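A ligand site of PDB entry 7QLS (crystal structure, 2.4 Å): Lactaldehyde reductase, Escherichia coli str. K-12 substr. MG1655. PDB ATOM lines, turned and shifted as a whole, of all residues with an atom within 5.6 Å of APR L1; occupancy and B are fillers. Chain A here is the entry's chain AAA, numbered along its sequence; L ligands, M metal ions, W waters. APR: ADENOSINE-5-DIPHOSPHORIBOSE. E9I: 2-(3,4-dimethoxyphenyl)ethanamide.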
ATOM      1  N   ASP A  39      26.077   4.929  -3.917  1.00  0.00           N
ATOM      2  CA  ASP A  39      24.782   4.259  -3.632  1.00  0.00           C
ATOM      3  C   ASP A  39      24.924   3.476  -2.316  1.00  0.00           C
ATOM      4  O   ASP A  39      26.051   3.408  -1.792  1.00  0.00           O
ATOM      5  CB  ASP A  39      24.312   3.397  -4.816  1.00  0.00           C
ATOM      6  CG  ASP A  39      25.305   2.342  -5.290  1.00  0.00           C
ATOM      7  OD1 ASP A  39      25.987   1.755  -4.433  1.00  0.00           O
ATOM      8  OD2 ASP A  39      25.379   2.124  -6.533  1.00  0.00           O
ATOM      9  N   THR A  41      24.694   0.190  -1.531  1.00  0.00           N
ATOM     10  CA  THR A  41      25.473  -1.088  -1.611  1.00  0.00           C
ATOM     11  C   THR A  41      26.969  -0.815  -1.369  1.00  0.00           C
ATOM     12  O   THR A  41      27.612  -1.629  -0.706  1.00  0.00           O
ATOM     13  CB  THR A  41      25.264  -1.787  -2.954  1.00  0.00           C
ATOM     14  OG1 THR A  41      23.872  -1.838  -3.220  1.00  0.00           O
ATOM     15  CG2 THR A  41      25.833  -3.190  -2.982  1.00  0.00           C
ATOM     16  N   LEU A  42      27.495   0.285  -1.890  1.00  0.00           N
ATOM     17  CA  LEU A  42      28.941   0.595  -1.834  1.00  0.00           C
ATOM     18  C   LEU A  42      29.318   1.126  -0.439  1.00  0.00           C
ATOM     19  O   LEU A  42      30.498   0.965  -0.064  1.00  0.00           O
ATOM     20  CB  LEU A  42      29.286   1.577  -2.957  1.00  0.00           C
ATOM     21  CG  LEU A  42      29.099   1.040  -4.381  1.00  0.00           C
ATOM     22  CD1 LEU A  42      29.142   2.167  -5.406  1.00  0.00           C
ATOM     23  CD2 LEU A  42      30.127  -0.029  -4.727  1.00  0.00           C
ATOM     24  N   CYS A  45      29.156  -2.424   1.685  1.00  0.00           N
ATOM     25  CA  CYS A  45      30.244  -3.380   1.335  1.00  0.00           C
ATOM     26  C   CYS A  45      31.620  -2.847   1.755  1.00  0.00           C
ATOM     27  O   CYS A  45      32.621  -3.551   1.515  1.00  0.00           O
ATOM     28  CB  CYS A  45      30.232  -3.698  -0.159  1.00  0.00           C
ATOM     29  SG  CYS A  45      28.955  -4.898  -0.636  1.00  0.00           S
ATOM     30  N   VAL A  47      33.284  -0.256   0.597  1.00  0.00           N
ATOM     31  CA  VAL A  47      34.041   0.244  -0.583  1.00  0.00           C
ATOM     32  C   VAL A  47      34.243   1.748  -0.398  1.00  0.00           C
ATOM     33  O   VAL A  47      35.385   2.218  -0.581  1.00  0.00           O
ATOM     34  CB  VAL A  47      33.334  -0.084  -1.905  1.00  0.00           C
ATOM     35  CG1 VAL A  47      33.917   0.677  -3.087  1.00  0.00           C
ATOM     36  CG2 VAL A  47      33.341  -1.578  -2.186  1.00  0.00           C
ATOM     37  N   PRO A  70      20.095   2.457  -9.610  1.00  0.00           N
ATOM     38  CA  PRO A  70      20.399   2.072 -10.998  1.00  0.00           C
ATOM     39  C   PRO A  70      19.527   2.850 -11.998  1.00  0.00           C
ATOM     40  O   PRO A  70      18.328   2.953 -11.782  1.00  0.00           O
ATOM     41  CB  PRO A  70      20.081   0.576 -11.043  1.00  0.00           C
ATOM     42  CG  PRO A  70      20.257   0.111  -9.612  1.00  0.00           C
ATOM     43  CD  PRO A  70      19.858   1.289  -8.744  1.00  0.00           C
ATOM     44  N   ASN A  71      20.134   3.351 -13.071  1.00  0.00           N
ATOM     45  CA  ASN A  71      19.461   4.181 -14.096  1.00  0.00           C
ATOM     46  C   ASN A  71      18.968   5.446 -13.393  1.00  0.00           C
ATOM     47  O   ASN A  71      17.755   5.654 -13.213  1.00  0.00           O
ATOM     48  CB  ASN A  71      18.368   3.395 -14.819  1.00  0.00           C
ATOM     49  CG  ASN A  71      18.872   2.084 -15.400  1.00  0.00           C
ATOM     50  OD1 ASN A  71      18.266   1.027 -15.212  1.00  0.00           O
ATOM     51  ND2 ASN A  71      19.986   2.114 -16.100  1.00  0.00           N
ATOM     52  N   PRO A  72      19.893   6.303 -12.932  1.00  0.00           N
ATOM     53  CA  PRO A  72      19.548   7.441 -12.092  1.00  0.00           C
ATOM     54  C   PRO A  72      18.467   8.315 -12.736  1.00  0.00           C
ATOM     55  O   PRO A  72      18.487   8.505 -13.954  1.00  0.00           O
ATOM     56  CB  PRO A  72      20.854   8.208 -11.917  1.00  0.00           C
ATOM     57  CG  PRO A  72      21.739   7.689 -13.023  1.00  0.00           C
ATOM     58  CD  PRO A  72      21.337   6.247 -13.195  1.00  0.00           C
ATOM     59  N   GLY A  96      31.385   4.728  -7.655  1.00  0.00           N
ATOM     60  CA  GLY A  96      30.445   3.736  -8.177  1.00  0.00           C
ATOM     61  C   GLY A  96      30.571   3.567  -9.684  1.00  0.00           C
ATOM     62  O   GLY A  96      31.522   4.143 -10.288  1.00  0.00           O
ATOM     63  N   GLY A  97      29.660   2.797 -10.270  1.00  0.00           N
ATOM     64  CA  GLY A  97      29.588   2.604 -11.736  1.00  0.00           C
ATOM     65  C   GLY A  97      28.964   3.804 -12.413  1.00  0.00           C
ATOM     66  O   GLY A  97      29.070   4.915 -11.854  1.00  0.00           O
ATOM     67  N   GLY A  98      28.352   3.599 -13.577  1.00  0.00           N
ATOM     68  CA  GLY A  98      27.721   4.665 -14.371  1.00  0.00           C
ATOM     69  C   GLY A  98      26.698   5.440 -13.554  1.00  0.00           C
ATOM     70  O   GLY A  98      26.660   6.684 -13.689  1.00  0.00           O
ATOM     71  N   SER A  99      25.885   4.772 -12.736  1.00  0.00           N
ATOM     72  CA  SER A  99      24.726   5.418 -12.071  1.00  0.00           C
ATOM     73  C   SER A  99      25.198   6.548 -11.169  1.00  0.00           C
ATOM     74  O   SER A  99      24.789   7.690 -11.377  1.00  0.00           O
ATOM     75  CB  SER A  99      23.867   4.400 -11.372  1.00  0.00           C
ATOM     76  OG  SER A  99      23.222   3.566 -12.325  1.00  0.00           O
ATOM     77  N   PRO A 100      26.084   6.328 -10.169  1.00  0.00           N
ATOM     78  CA  PRO A 100      26.583   7.427  -9.342  1.00  0.00           C
ATOM     79  C   PRO A 100      27.409   8.458 -10.111  1.00  0.00           C
ATOM     80  O   PRO A 100      27.246   9.634  -9.886  1.00  0.00           O
ATOM     81  CB  PRO A 100      27.453   6.721  -8.285  1.00  0.00           C
ATOM     82  CG  PRO A 100      26.952   5.291  -8.300  1.00  0.00           C
ATOM     83  CD  PRO A 100      26.623   5.028  -9.742  1.00  0.00           C
ATOM     84  N   ASP A 102      27.305   9.301 -13.323  1.00  0.00           N
ATOM     85  CA  ASP A 102      26.383  10.071 -14.187  1.00  0.00           C
ATOM     86  C   ASP A 102      25.552  11.015 -13.296  1.00  0.00           C
ATOM     87  O   ASP A 102      25.334  12.183 -13.696  1.00  0.00           O
ATOM     88  CB  ASP A 102      25.525   9.147 -15.053  1.00  0.00           C
ATOM     89  CG  ASP A 102      26.270   8.485 -16.212  1.00  0.00           C
ATOM     90  OD1 ASP A 102      27.526   8.597 -16.274  1.00  0.00           O
ATOM     91  OD2 ASP A 102      25.589   7.855 -17.062  1.00  0.00           O
ATOM     92  N   THR A 140      33.771   1.679  -9.710  1.00  0.00           N
ATOM     93  CA  THR A 140      33.631   0.420  -8.952  1.00  0.00           C
ATOM     94  C   THR A 140      33.038  -0.677  -9.844  1.00  0.00           C
ATOM     95  O   THR A 140      32.835  -1.787  -9.330  1.00  0.00           O
ATOM     96  CB  THR A 140      32.772   0.644  -7.702  1.00  0.00           C
ATOM     97  OG1 THR A 140      31.436   0.853  -8.121  1.00  0.00           O
ATOM     98  CG2 THR A 140      33.236   1.829  -6.886  1.00  0.00           C
ATOM     99  N   THR A 141      32.779  -0.376 -11.126  1.00  0.00           N
ATOM    100  CA  THR A 141      32.426  -1.378 -12.158  1.00  0.00           C
ATOM    101  C   THR A 141      33.442  -1.275 -13.302  1.00  0.00           C
ATOM    102  O   THR A 141      34.063  -0.221 -13.451  1.00  0.00           O
ATOM    103  CB  THR A 141      30.974  -1.272 -12.632  1.00  0.00           C
ATOM    104  OG1 THR A 141      30.773  -0.086 -13.423  1.00  0.00           O
ATOM    105  CG2 THR A 141      29.999  -1.317 -11.489  1.00  0.00           C
ATOM    106  N   GLY A 143      33.392  -1.554 -16.962  1.00  0.00           N
ATOM    107  CA  GLY A 143      32.021  -1.088 -17.155  1.00  0.00           C
ATOM    108  C   GLY A 143      31.985   0.179 -17.983  1.00  0.00           C
ATOM    109  O   GLY A 143      32.393   0.071 -19.131  1.00  0.00           O
ATOM    110  N   THR A 144      31.474   1.293 -17.441  1.00  0.00           N
ATOM    111  CA  THR A 144      30.841   2.373 -18.236  1.00  0.00           C
ATOM    112  C   THR A 144      31.876   3.356 -18.765  1.00  0.00           C
ATOM    113  O   THR A 144      31.576   4.036 -19.741  1.00  0.00           O
ATOM    114  CB  THR A 144      29.754   3.136 -17.458  1.00  0.00           C
ATOM    115  OG1 THR A 144      30.393   3.883 -16.420  1.00  0.00           O
ATOM    116  CG2 THR A 144      28.710   2.210 -16.872  1.00  0.00           C
ATOM    117  N   VAL A 153      23.855   9.665 -18.655  1.00  0.00           N
ATOM    118  CA  VAL A 153      22.507   9.188 -19.063  1.00  0.00           C
ATOM    119  C   VAL A 153      21.585   9.220 -17.831  1.00  0.00           C
ATOM    120  O   VAL A 153      21.867   8.515 -16.837  1.00  0.00           O
ATOM    121  CB  VAL A 153      22.586   7.794 -19.725  1.00  0.00           C
ATOM    122  CG1 VAL A 153      21.252   7.353 -20.266  1.00  0.00           C
ATOM    123  CG2 VAL A 153      23.626   7.787 -20.823  1.00  0.00           C
ATOM    124  N   LYS A 162      15.384   7.202 -21.184  1.00  0.00           N
ATOM    125  CA  LYS A 162      16.748   7.652 -20.846  1.00  0.00           C
ATOM    126  C   LYS A 162      17.190   8.661 -21.904  1.00  0.00           C
ATOM    127  O   LYS A 162      16.967   8.394 -23.101  1.00  0.00           O
ATOM    128  CB  LYS A 162      17.700   6.462 -20.762  1.00  0.00           C
ATOM    129  CG  LYS A 162      17.588   5.643 -19.486  1.00  0.00           C
ATOM    130  CD  LYS A 162      18.129   4.233 -19.590  1.00  0.00           C
ATOM    131  CE  LYS A 162      19.639   4.135 -19.629  1.00  0.00           C
ATOM    132  NZ  LYS A 162      20.243   4.406 -18.302  1.00  0.00           N
ATOM    133  N   MET A 181      38.780  -1.533  -6.008  1.00  0.00           N
ATOM    134  CA  MET A 181      37.427  -0.949  -5.803  1.00  0.00           C
ATOM    135  C   MET A 181      36.373  -1.785  -6.520  1.00  0.00           C
ATOM    136  O   MET A 181      35.177  -1.608  -6.217  1.00  0.00           O
ATOM    137  CB  MET A 181      37.361   0.491  -6.334  1.00  0.00           C
ATOM    138  CG  MET A 181      38.248   1.448  -5.563  1.00  0.00           C
ATOM    139  SD  MET A 181      37.596   1.763  -3.907  1.00  0.00           S
ATOM    140  CE  MET A 181      39.130   1.954  -3.016  1.00  0.00           C
ATOM    141  N   MET A 182      36.805  -2.691  -7.415  1.00  0.00           N
ATOM    142  CA  MET A 182      35.957  -3.427  -8.378  1.00  0.00           C
ATOM    143  C   MET A 182      35.778  -4.895  -7.965  1.00  0.00           C
ATOM    144  O   MET A 182      34.824  -5.521  -8.463  1.00  0.00           O
ATOM    145  CB  MET A 182      36.568  -3.371  -9.778  1.00  0.00           C
ATOM    146  CG  MET A 182      36.553  -1.973 -10.380  1.00  0.00           C
ATOM    147  SD  MET A 182      37.592  -1.872 -11.864  1.00  0.00           S
ATOM    148  CE  MET A 182      37.622  -0.098 -12.111  1.00  0.00           C
ATOM    149  N   ASP A 183      36.643  -5.425  -7.100  1.00  0.00           N
ATOM    150  CA  ASP A 183      36.712  -6.897  -6.813  1.00  0.00           C
ATOM    151  C   ASP A 183      35.378  -7.389  -6.238  1.00  0.00           C
ATOM    152  O   ASP A 183      35.065  -8.563  -6.457  1.00  0.00           O
ATOM    153  CB  ASP A 183      37.880  -7.237  -5.884  1.00  0.00           C
ATOM    154  CG  ASP A 183      39.252  -7.135  -6.536  1.00  0.00           C
ATOM    155  OD1 ASP A 183      39.328  -7.266  -7.778  1.00  0.00           O
ATOM    156  OD2 ASP A 183      40.230  -6.932  -5.795  1.00  0.00           O
ATOM    157  N   GLY A 184      34.635  -6.533  -5.535  1.00  0.00           N
ATOM    158  CA  GLY A 184      33.401  -6.881  -4.792  1.00  0.00           C
ATOM    159  C   GLY A 184      32.179  -7.033  -5.685  1.00  0.00           C
ATOM    160  O   GLY A 184      31.136  -7.485  -5.179  1.00  0.00           O
ATOM    161  N   MET A 185      32.264  -6.651  -6.970  1.00  0.00           N
ATOM    162  CA  MET A 185      31.223  -6.943  -7.979  1.00  0.00           C
ATOM    163  C   MET A 185      30.895  -8.432  -7.904  1.00  0.00           C
ATOM    164  O   MET A 185      31.788  -9.262  -8.025  1.00  0.00           O
ATOM    165  CB  MET A 185      31.720  -6.657  -9.401  1.00  0.00           C
ATOM    166  CG  MET A 185      31.815  -5.190  -9.742  1.00  0.00           C
ATOM    167  SD  MET A 185      32.576  -4.929 -11.367  1.00  0.00           S
ATOM    168  CE  MET A 185      31.110  -4.957 -12.367  1.00  0.00           C
ATOM    169  N   PRO A 186      29.610  -8.814  -7.713  1.00  0.00           N
ATOM    170  CA  PRO A 186      29.178 -10.177  -7.989  1.00  0.00           C
ATOM    171  C   PRO A 186      29.513 -10.578  -9.423  1.00  0.00           C
ATOM    172  O   PRO A 186      29.523  -9.743 -10.328  1.00  0.00           O
ATOM    173  CB  PRO A 186      27.653 -10.151  -7.767  1.00  0.00           C
ATOM    174  CG  PRO A 186      27.447  -8.963  -6.827  1.00  0.00           C
ATOM    175  CD  PRO A 186      28.509  -7.966  -7.216  1.00  0.00           C
ATOM    176  N   LEU A 189      27.551  -9.024 -12.329  1.00  0.00           N
ATOM    177  CA  LEU A 189      27.822  -7.570 -12.520  1.00  0.00           C
ATOM    178  C   LEU A 189      29.116  -7.385 -13.312  1.00  0.00           C
ATOM    179  O   LEU A 189      29.171  -6.497 -14.181  1.00  0.00           O
ATOM    180  CB  LEU A 189      27.914  -6.886 -11.146  1.00  0.00           C
ATOM    181  CG  LEU A 189      27.886  -5.364 -11.161  1.00  0.00           C
ATOM    182  CD1 LEU A 189      26.681  -4.819 -11.914  1.00  0.00           C
ATOM    183  CD2 LEU A 189      27.905  -4.823  -9.728  1.00  0.00           C
ATOM    184  N   THR A 193      28.766  -5.467 -16.958  1.00  0.00           N
ATOM    185  CA  THR A 193      29.518  -4.202 -17.156  1.00  0.00           C
ATOM    186  C   THR A 193      30.710  -4.478 -18.091  1.00  0.00           C
ATOM    187  O   THR A 193      31.074  -3.558 -18.869  1.00  0.00           O
ATOM    188  CB  THR A 193      29.896  -3.599 -15.788  1.00  0.00           C
ATOM    189  OG1 THR A 193      30.786  -4.502 -15.139  1.00  0.00           O
ATOM    190  CG2 THR A 193      28.694  -3.318 -14.920  1.00  0.00           C
ATOM    191  N   ASP A 196      29.319  -4.357 -21.533  1.00  0.00           N
ATOM    192  CA  ASP A 196      29.021  -2.929 -21.813  1.00  0.00           C
ATOM    193  C   ASP A 196      30.307  -2.279 -22.343  1.00  0.00           C
ATOM    194  O   ASP A 196      30.239  -1.577 -23.376  1.00  0.00           O
ATOM    195  CB  ASP A 196      28.405  -2.240 -20.591  1.00  0.00           C
ATOM    196  CG  ASP A 196      28.156  -0.743 -20.748  1.00  0.00           C
ATOM    197  OD1 ASP A 196      27.718  -0.322 -21.835  1.00  0.00           O
ATOM    198  OD2 ASP A 196      28.384  -0.017 -19.760  1.00  0.00           O
ATOM    199  N   HIS A 267      18.856   1.635 -24.316  1.00  0.00           N
ATOM    200  CA  HIS A 267      18.359   2.743 -23.458  1.00  0.00           C
ATOM    201  C   HIS A 267      16.862   2.609 -23.212  1.00  0.00           C
ATOM    202  O   HIS A 267      16.429   2.748 -22.075  1.00  0.00           O
ATOM    203  CB  HIS A 267      18.768   4.115 -24.030  1.00  0.00           C
ATOM    204  CG  HIS A 267      20.214   4.420 -23.838  1.00  0.00           C
ATOM    205  ND1 HIS A 267      20.802   5.547 -24.392  1.00  0.00           N
ATOM    206  CD2 HIS A 267      21.185   3.764 -23.158  1.00  0.00           C
ATOM    207  CE1 HIS A 267      22.077   5.562 -24.058  1.00  0.00           C
ATOM    208  NE2 HIS A 267      22.339   4.467 -23.308  1.00  0.00           N
ATOM    209  N   HIS A 277      21.888  -1.947 -17.941  1.00  0.00           N
ATOM    210  CA  HIS A 277      22.452  -1.436 -19.215  1.00  0.00           C
ATOM    211  C   HIS A 277      23.344  -2.493 -19.897  1.00  0.00           C
ATOM    212  O   HIS A 277      23.214  -2.685 -21.122  1.00  0.00           O
ATOM    213  CB  HIS A 277      23.200  -0.126 -18.919  1.00  0.00           C
ATOM    214  CG  HIS A 277      23.920   0.453 -20.089  1.00  0.00           C
ATOM    215  ND1 HIS A 277      23.254   0.988 -21.181  1.00  0.00           N
ATOM    216  CD2 HIS A 277      25.232   0.630 -20.327  1.00  0.00           C
ATOM    217  CE1 HIS A 277      24.123   1.450 -22.035  1.00  0.00           C
ATOM    218  NE2 HIS A 277      25.351   1.250 -21.532  1.00  0.00           N
ATOM    219  N   GLY A 278      24.227  -3.144 -19.124  1.00  0.00           N
ATOM    220  CA  GLY A 278      25.199  -4.132 -19.614  1.00  0.00           C
ATOM    221  C   GLY A 278      24.531  -5.388 -20.154  1.00  0.00           C
ATOM    222  O   GLY A 278      25.004  -5.906 -21.203  1.00  0.00           O
HETATM  223  N1  APR L   1      30.452  -4.022  -5.546  1.00  0.00           N
HETATM  224  C2  APR L   1      29.163  -4.303  -5.327  1.00  0.00           C
HETATM  225  N3  APR L   1      28.073  -3.805  -5.905  1.00  0.00           N
HETATM  226  C4  APR L   1      28.406  -2.878  -6.816  1.00  0.00           C
HETATM  227  C5  APR L   1      29.678  -2.473  -7.151  1.00  0.00           C
HETATM  228  C6  APR L   1      30.755  -3.080  -6.483  1.00  0.00           C
HETATM  229  N6  APR L   1      32.034  -2.801  -6.703  1.00  0.00           N
HETATM  230  N7  APR L   1      29.623  -1.500  -8.143  1.00  0.00           N
HETATM  231  C8  APR L   1      28.339  -1.335  -8.383  1.00  0.00           C
HETATM  232  N9  APR L   1      27.551  -2.151  -7.598  1.00  0.00           N
HETATM  233  C1' APR L   1      26.087  -2.254  -7.605  1.00  0.00           C
HETATM  234  C2' APR L   1      25.365  -0.928  -7.422  1.00  0.00           C
HETATM  235  O2' APR L   1      25.254  -0.621  -6.048  1.00  0.00           O
HETATM  236  C3' APR L   1      24.012  -1.238  -8.072  1.00  0.00           C
HETATM  237  O3' APR L   1      23.158  -1.883  -7.145  1.00  0.00           O
HETATM  238  O4' APR L   1      25.680  -2.738  -8.868  1.00  0.00           O
HETATM  239  C4' APR L   1      24.399  -2.171  -9.232  1.00  0.00           C
HETATM  240  C5' APR L   1      24.495  -1.522 -10.591  1.00  0.00           C
HETATM  241  O5' APR L   1      25.282  -0.295 -10.505  1.00  0.00           O
HETATM  242  PA  APR L   1      25.333   0.737 -11.723  1.00  0.00           P
HETATM  243  O1A APR L   1      26.114   1.947 -11.316  1.00  0.00           O
HETATM  244  O2A APR L   1      23.960   0.929 -12.284  1.00  0.00           O
HETATM  245  O3A APR L   1      26.218  -0.070 -12.804  1.00  0.00           O
HETATM  246  PB  APR L   1      26.856   0.373 -14.203  1.00  0.00           P
HETATM  247  O1B APR L   1      28.265   0.780 -13.966  1.00  0.00           O
HETATM  248  O2B APR L   1      26.576  -0.694 -15.218  1.00  0.00           O
HETATM  249  O5D APR L   1      26.008   1.672 -14.563  1.00  0.00           O
HETATM  250  C5D APR L   1      25.209   1.718 -15.767  1.00  0.00           C
HETATM  251  O4D APR L   1      25.575   3.942 -16.608  1.00  0.00           O
HETATM  252  O1D APR L   1      25.948   4.362 -18.850  1.00  0.00           O
HETATM  253  C1D APR L   1      25.012   4.423 -17.827  1.00  0.00           C
HETATM  254  O2D APR L   1      22.798   4.075 -18.919  1.00  0.00           O
HETATM  255  C2D APR L   1      23.811   3.515 -18.103  1.00  0.00           C
HETATM  256  O3D APR L   1      22.476   4.209 -16.119  1.00  0.00           O
HETATM  257  C3D APR L   1      23.309   3.200 -16.681  1.00  0.00           C
HETATM  258  C4D APR L   1      24.630   3.102 -15.912  1.00  0.00           C
HETATM  259  N1  E9I L   2      28.678   5.340 -21.764  1.00  0.00           N
HETATM  260  C7  E9I L   2      26.809   7.527 -26.115  1.00  0.00           C
HETATM  261  C8  E9I L   2      27.447   5.216 -22.235  1.00  0.00           C
HETATM  262  C9  E9I L   2      30.211  10.170 -24.362  1.00  0.00           C
HETATM  263  O1  E9I L   2      28.897  10.222 -24.923  1.00  0.00           O
HETATM  264  C1  E9I L   2      27.064   7.253 -23.724  1.00  0.00           C
HETATM  265  C5  E9I L   2      26.545   6.828 -24.940  1.00  0.00           C
HETATM  266  C6  E9I L   2      27.602   8.654 -26.072  1.00  0.00           C
HETATM  267  C4  E9I L   2      28.150   9.085 -24.851  1.00  0.00           C
HETATM  268  C3  E9I L   2      27.881   8.370 -23.692  1.00  0.00           C
HETATM  269  O3  E9I L   2      26.928   4.124 -22.493  1.00  0.00           O
HETATM  270  C2  E9I L   2      26.691   6.549 -22.438  1.00  0.00           C
HETATM  271  O2  E9I L   2      27.912   9.421 -27.167  1.00  0.00           O
HETATM  272  C10 E9I L   2      26.838   9.904 -27.958  1.00  0.00           C
HETATM  273 FE    FE M   1      27.245   1.820 -22.220  1.00  0.00          FE
HETATM  274  O   HOH W   1      24.273   4.419 -21.191  1.00  0.00           O
HETATM  275  O   HOH W   2      26.122  -5.603  -5.219  1.00  0.00           O
HETATM  276  O   HOH W   3      27.779   2.378 -20.213  1.00  0.00           O
HETATM  277  O   HOH W   4      23.410   6.611 -15.947  1.00  0.00           O
HETATM  278  O   HOH W   5      27.329   1.939  -8.867  1.00  0.00           O
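The side-chain hydroxyl of Ser 99 sits at hydrogen-bond distance from the backbone NH of Asn 71 (3.2 Å).
N of Leu 42 sits close to OD1 of Asp 39, at 3.3 Å.
The side-chain hydroxyl (OG1) of Thr 140 lies within hydrogen-bond range of the backbone NH (N) of Gly 97, 3.4 Å away.
The backbone NH (N) of Thr 140 is in hydrogen-bond range of the backbone carbonyl oxygen (O) of Gly 96, 3.4 Å away.
The side-chain hydroxyl of Thr 193 is in hydrogen-bond range of the backbone carbonyl oxygen of Leu 189, at 2.7 Å.
The backbone carbonyl oxygen (O) of Thr 41 sits close to the side-chain sulfur (SG) of Cys 45 (3.5 Å).
O of Leu 42 is in hydrogen-bond range of N of Val 47.
The backbone NH (N) of Val 153 lies within hydrogen-bond range of the side-chain carboxylate (OD2) of Asp 102 (3.0 Å).
Water W4 lies within hydrogen-bond range of an oxygen (O3D) of APR L1 (2.6 Å), the backbone carbonyl oxygen (O) of Val 153 (2.6 Å) and the side-chain carboxylate (OD2) of Asp 102 (2.7 Å).
Water W1 lies within hydrogen-bond range of an oxygen (O2D) of APR L1 (2.7 Å) and a ring nitrogen (NE2) of His 267 (2.9 Å).
Water W5 lies within hydrogen-bond range of O1A of APR L1, N of Gly 97 and OD2 of Asp 39.
Water W3 lies within hydrogen-bond range of the side-chain carboxylate (OD2) of Asp 196, an oxygen (O1D) of APR L1 and a nitrogen (N1) of E9I L2.
O2D of APR L1 sits at hydrogen-bond distance from NZ of Lys 162, 2.6 Å away.
An oxygen (O1B) of APR L1 sits at hydrogen-bond distance from the side-chain hydroxyl (OG1) of Thr 141 (2.7 Å).
N of Ser 99 lies within hydrogen-bond range of O1A of APR L1, 3.2 Å away.
OG of Ser 99 sits at hydrogen-bond distance from O2A of APR L1 (2.7 Å).
O2' of APR L1 is in hydrogen-bond range of OD2 of Asp 39, 2.8 Å away.
The backbone NH (N) of Gly 98 sits at hydrogen-bond distance from an oxygen (O1B) of APR L1 (2.8 Å).
O of Thr 140 lies within hydrogen-bond range of N6 of APR L1 (2.9 Å).
The side-chain hydroxyl (OG1) of Thr 140 lies within hydrogen-bond range of a nitrogen (N7) of APR L1 (3.0 Å).
The side-chain amide nitrogen (ND2) of Asn 71 is in hydrogen-bond range of an oxygen (O3D) of APR L1 (3.3 Å).
OG1 of Thr 41 sits close to O2' of APR L1.
A nitrogen (N6) of APR L1 lies within hydrogen-bond range of the backbone carbonyl oxygen of Met 181.
The backbone NH (N) of Met 185 is in hydrogen-bond range of a nitrogen (N1) of APR L1, at 3.5 Å.
Leu 42 touches APR L1 (CD2 to C5, 3.5 Å).
Pro 70 touches APR L1.
CD of Pro 72 touches O3D of APR L1, at 3.7 Å.
Gly 97 touches APR L1.
Pro 100 touches APR L1 (CD to O1A, 3.5 Å).
Asp 102 touches APR L1.
Thr 144 touches APR L1.
CB of Val 153 touches O2D of APR L1, 3.8 Å away.
Gly 184 touches APR L1 (C to N1, 3.5 Å).
CD2 of Leu 189 touches O4' of APR L1 (3.2 Å).
CG2 of Thr 193 touches O2B of APR L1, 3.4 Å away.
His 277 touches APR L1 (CG to C2D, 3.7 Å).
Hydrophobic or aromatic side chains within 4 Å of APR L1: Leu 42, Pro 72, Pro 100, Val 153, Met 185, Leu 189 and His 277.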
